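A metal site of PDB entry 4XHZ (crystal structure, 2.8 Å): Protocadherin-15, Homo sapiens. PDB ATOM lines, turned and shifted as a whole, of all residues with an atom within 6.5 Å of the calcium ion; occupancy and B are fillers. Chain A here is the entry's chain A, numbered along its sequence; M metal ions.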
ATOM      1  N   ASN A 106      -9.003 -11.741  -3.619  1.00  0.00           N
ATOM      2  CA  ASN A 106      -8.251 -12.967  -3.772  1.00  0.00           C
ATOM      3  C   ASN A 106      -8.760 -13.725  -5.032  1.00  0.00           C
ATOM      4  O   ASN A 106      -9.960 -13.978  -5.153  1.00  0.00           O
ATOM      5  CB  ASN A 106      -8.347 -13.781  -2.466  1.00  0.00           C
ATOM      6  CG  ASN A 106      -7.889 -15.211  -2.610  1.00  0.00           C
ATOM      7  OD1 ASN A 106      -6.736 -15.494  -2.977  1.00  0.00           O
ATOM      8  ND2 ASN A 106      -8.781 -16.148  -2.281  1.00  0.00           N
ATOM      9  N   ASP A 107      -7.863 -14.054  -5.966  1.00  0.00           N
ATOM     10  CA  ASP A 107      -8.271 -14.680  -7.240  1.00  0.00           C
ATOM     11  C   ASP A 107      -8.200 -16.204  -7.297  1.00  0.00           C
ATOM     12  O   ASP A 107      -9.102 -16.863  -7.829  1.00  0.00           O
ATOM     13  CB  ASP A 107      -7.491 -14.098  -8.414  1.00  0.00           C
ATOM     14  CG  ASP A 107      -7.949 -12.726  -8.779  1.00  0.00           C
ATOM     15  OD1 ASP A 107      -7.816 -11.821  -7.935  1.00  0.00           O
ATOM     16  OD2 ASP A 107      -8.459 -12.537  -9.899  1.00  0.00           O
ATOM     17  N   TYR A 108      -7.125 -16.777  -6.768  1.00  0.00           N
ATOM     18  CA  TYR A 108      -6.878 -18.198  -6.939  1.00  0.00           C
ATOM     19  C   TYR A 108      -6.837 -18.984  -5.651  1.00  0.00           C
ATOM     20  O   TYR A 108      -6.401 -18.465  -4.605  1.00  0.00           O
ATOM     21  CB  TYR A 108      -5.573 -18.411  -7.683  1.00  0.00           C
ATOM     22  CG  TYR A 108      -5.367 -17.495  -8.842  1.00  0.00           C
ATOM     23  CD1 TYR A 108      -6.078 -17.670 -10.024  1.00  0.00           C
ATOM     24  CD2 TYR A 108      -4.457 -16.443  -8.768  1.00  0.00           C
ATOM     25  CE1 TYR A 108      -5.874 -16.833 -11.101  1.00  0.00           C
ATOM     26  CE2 TYR A 108      -4.260 -15.605  -9.840  1.00  0.00           C
ATOM     27  CZ  TYR A 108      -4.970 -15.800 -10.999  1.00  0.00           C
ATOM     28  OH  TYR A 108      -4.768 -14.962 -12.063  1.00  0.00           O
ATOM     29  N   PRO A 109      -7.277 -20.250  -5.714  1.00  0.00           N
ATOM     30  CA  PRO A 109      -7.090 -21.133  -4.589  1.00  0.00           C
ATOM     31  C   PRO A 109      -5.674 -21.656  -4.638  1.00  0.00           C
ATOM     32  O   PRO A 109      -4.999 -21.575  -5.693  1.00  0.00           O
ATOM     33  CB  PRO A 109      -8.058 -22.274  -4.894  1.00  0.00           C
ATOM     34  CG  PRO A 109      -8.077 -22.357  -6.393  1.00  0.00           C
ATOM     35  CD  PRO A 109      -7.789 -20.956  -6.897  1.00  0.00           C
ATOM     36  N   PRO A 110      -5.180 -22.175  -3.510  1.00  0.00           N
ATOM     37  CA  PRO A 110      -3.943 -22.922  -3.521  1.00  0.00           C
ATOM     38  C   PRO A 110      -4.112 -24.186  -4.346  1.00  0.00           C
ATOM     39  O   PRO A 110      -5.222 -24.767  -4.409  1.00  0.00           O
ATOM     40  CB  PRO A 110      -3.741 -23.268  -2.044  1.00  0.00           C
ATOM     41  CG  PRO A 110      -4.468 -22.204  -1.312  1.00  0.00           C
ATOM     42  CD  PRO A 110      -5.677 -21.936  -2.151  1.00  0.00           C
ATOM     43  N   ASP A 138       0.174 -20.873  -4.271  1.00  0.00           N
ATOM     44  CA  ASP A 138      -0.914 -19.943  -4.497  1.00  0.00           C
ATOM     45  C   ASP A 138      -0.485 -18.884  -5.474  1.00  0.00           C
ATOM     46  O   ASP A 138       0.461 -18.133  -5.232  1.00  0.00           O
ATOM     47  CB  ASP A 138      -1.365 -19.307  -3.186  1.00  0.00           C
ATOM     48  CG  ASP A 138      -2.723 -18.652  -3.303  1.00  0.00           C
ATOM     49  OD1 ASP A 138      -2.817 -17.579  -3.927  1.00  0.00           O
ATOM     50  OD2 ASP A 138      -3.699 -19.206  -2.780  1.00  0.00           O
ATOM     51  N   ALA A 139      -1.202 -18.826  -6.593  1.00  0.00           N
ATOM     52  CA  ALA A 139      -0.873 -17.910  -7.678  1.00  0.00           C
ATOM     53  C   ALA A 139      -1.017 -16.385  -7.355  1.00  0.00           C
ATOM     54  O   ALA A 139      -0.511 -15.560  -8.092  1.00  0.00           O
ATOM     55  CB  ALA A 139      -1.669 -18.279  -8.920  1.00  0.00           C
ATOM     56  N   ASP A 140      -1.702 -16.023  -6.273  1.00  0.00           N
ATOM     57  CA  ASP A 140      -1.894 -14.603  -5.934  1.00  0.00           C
ATOM     58  C   ASP A 140      -0.572 -13.915  -5.538  1.00  0.00           C
ATOM     59  O   ASP A 140       0.383 -14.579  -5.138  1.00  0.00           O
ATOM     60  CB  ASP A 140      -2.916 -14.451  -4.816  1.00  0.00           C
ATOM     61  CG  ASP A 140      -4.335 -14.799  -5.264  1.00  0.00           C
ATOM     62  OD1 ASP A 140      -4.991 -13.935  -5.880  1.00  0.00           O
ATOM     63  OD2 ASP A 140      -4.777 -15.929  -4.993  1.00  0.00           O
ATOM     64  N   PRO A 145      -1.628 -12.076   2.654  1.00  0.00           N
ATOM     65  CA  PRO A 145      -2.534 -13.057   3.256  1.00  0.00           C
ATOM     66  C   PRO A 145      -3.320 -13.876   2.204  1.00  0.00           C
ATOM     67  O   PRO A 145      -3.817 -14.970   2.513  1.00  0.00           O
ATOM     68  CB  PRO A 145      -3.462 -12.184   4.114  1.00  0.00           C
ATOM     69  CG  PRO A 145      -2.619 -11.010   4.481  1.00  0.00           C
ATOM     70  CD  PRO A 145      -1.790 -10.735   3.247  1.00  0.00           C
ATOM     71  N   ALA A 146      -3.429 -13.384   0.985  1.00  0.00           N
ATOM     72  CA  ALA A 146      -4.188 -14.084  -0.045  1.00  0.00           C
ATOM     73  C   ALA A 146      -3.363 -15.176  -0.771  1.00  0.00           C
ATOM     74  O   ALA A 146      -3.914 -16.002  -1.511  1.00  0.00           O
ATOM     75  CB  ALA A 146      -4.772 -13.103  -1.054  1.00  0.00           C
ATOM     76  N   SER A 147      -2.052 -15.173  -0.556  1.00  0.00           N
ATOM     77  CA  SER A 147      -1.194 -16.225  -1.098  1.00  0.00           C
ATOM     78  C   SER A 147      -0.435 -16.919   0.037  1.00  0.00           C
ATOM     79  O   SER A 147       0.694 -17.378  -0.142  1.00  0.00           O
ATOM     80  CB  SER A 147      -0.208 -15.650  -2.110  1.00  0.00           C
ATOM     81  OG  SER A 147       0.863 -15.005  -1.451  1.00  0.00           O
ATOM     82  N   ARG A 148      -1.065 -16.963   1.207  1.00  0.00           N
ATOM     83  CA  ARG A 148      -0.481 -17.620   2.364  1.00  0.00           C
ATOM     84  C   ARG A 148      -1.205 -18.926   2.587  1.00  0.00           C
ATOM     85  O   ARG A 148      -2.407 -18.961   2.877  1.00  0.00           O
ATOM     86  CB  ARG A 148      -0.589 -16.726   3.588  1.00  0.00           C
ATOM     87  CG  ARG A 148      -0.419 -17.443   4.913  1.00  0.00           C
ATOM     88  CD  ARG A 148       1.026 -17.509   5.336  1.00  0.00           C
ATOM     89  NE  ARG A 148       1.141 -17.405   6.796  1.00  0.00           N
ATOM     90  CZ  ARG A 148       1.212 -18.442   7.630  1.00  0.00           C
ATOM     91  NH1 ARG A 148       1.211 -19.695   7.175  1.00  0.00           N
ATOM     92  NH2 ARG A 148       1.302 -18.218   8.943  1.00  0.00           N
ATOM     93  N   ASP A 196      -6.177 -20.510   1.739  1.00  0.00           N
ATOM     94  CA  ASP A 196      -5.418 -19.271   1.936  1.00  0.00           C
ATOM     95  C   ASP A 196      -6.081 -18.340   2.944  1.00  0.00           C
ATOM     96  O   ASP A 196      -6.969 -18.747   3.717  1.00  0.00           O
ATOM     97  CB  ASP A 196      -5.202 -18.540   0.605  1.00  0.00           C
ATOM     98  CG  ASP A 196      -6.522 -18.128  -0.080  1.00  0.00           C
ATOM     99  OD1 ASP A 196      -7.586 -18.049   0.592  1.00  0.00           O
ATOM    100  OD2 ASP A 196      -6.476 -17.881  -1.319  1.00  0.00           O
ATOM    101  N   ASP A 197      -5.670 -17.082   2.929  1.00  0.00           N
ATOM    102  CA  ASP A 197      -6.222 -16.092   3.841  1.00  0.00           C
ATOM    103  C   ASP A 197      -6.559 -14.798   3.077  1.00  0.00           C
ATOM    104  O   ASP A 197      -6.050 -13.715   3.375  1.00  0.00           O
ATOM    105  CB  ASP A 197      -5.224 -15.814   4.967  1.00  0.00           C
ATOM    106  CG  ASP A 197      -5.884 -15.261   6.197  1.00  0.00           C
ATOM    107  OD1 ASP A 197      -7.090 -15.518   6.371  1.00  0.00           O
ATOM    108  OD2 ASP A 197      -5.210 -14.557   6.994  1.00  0.00           O
ATOM    109  N   GLY A 198      -7.415 -14.927   2.067  1.00  0.00           N
ATOM    110  CA  GLY A 198      -7.770 -13.803   1.248  1.00  0.00           C
ATOM    111  C   GLY A 198      -9.234 -13.505   1.403  1.00  0.00           C
ATOM    112  O   GLY A 198      -9.960 -14.230   2.089  1.00  0.00           O
ATOM    113  N   MET A 202     -10.155 -19.122  -0.296  1.00  0.00           N
ATOM    114  CA  MET A 202     -10.268 -20.153  -1.305  1.00  0.00           C
ATOM    115  C   MET A 202      -9.439 -21.368  -0.917  1.00  0.00           C
ATOM    116  O   MET A 202      -8.466 -21.264  -0.144  1.00  0.00           O
ATOM    117  CB  MET A 202      -9.879 -19.599  -2.676  1.00  0.00           C
ATOM    118  CG  MET A 202     -10.866 -18.573  -3.231  1.00  0.00           C
ATOM    119  SD  MET A 202     -10.383 -17.800  -4.800  1.00  0.00           S
ATOM    120  CE  MET A 202     -10.675 -19.148  -5.956  1.00  0.00           C
HETATM  121 CA    CA M   1      -5.180 -17.298  -3.179  1.00  0.00          CA
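The side-chain carboxylate (OD1) of Asp 140 sits at hydrogen-bond distance from the backbone NH (N) of Asp 107 (2.9 Å). The backbone NH (N) of Gly 198 is in hydrogen-bond range of the side-chain carboxylate (OD1) of Asp 196 (3.5 Å). The backbone NH (N) of Met 202 sits at hydrogen-bond distance from the side-chain carboxylate (OD1) of Asp 196, 2.9 Å away. ND2 of Asn 106 lies close to SD of Met 202, at 3.4 Å.
The calcium ion is bound by O of Tyr 108 (2.2 Å), OD2 of Asp 140 (2.3 Å), OD2 of Asp 196 (2.3 Å), OD1 of Asn 106 (2.4 Å), OD2 of Asp 138 (2.4 Å), O of Ala 146 (2.5 Å) and OD1 of Asp 138 (2.5 Å). The calcium ion has seven donor atoms within binding distance.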
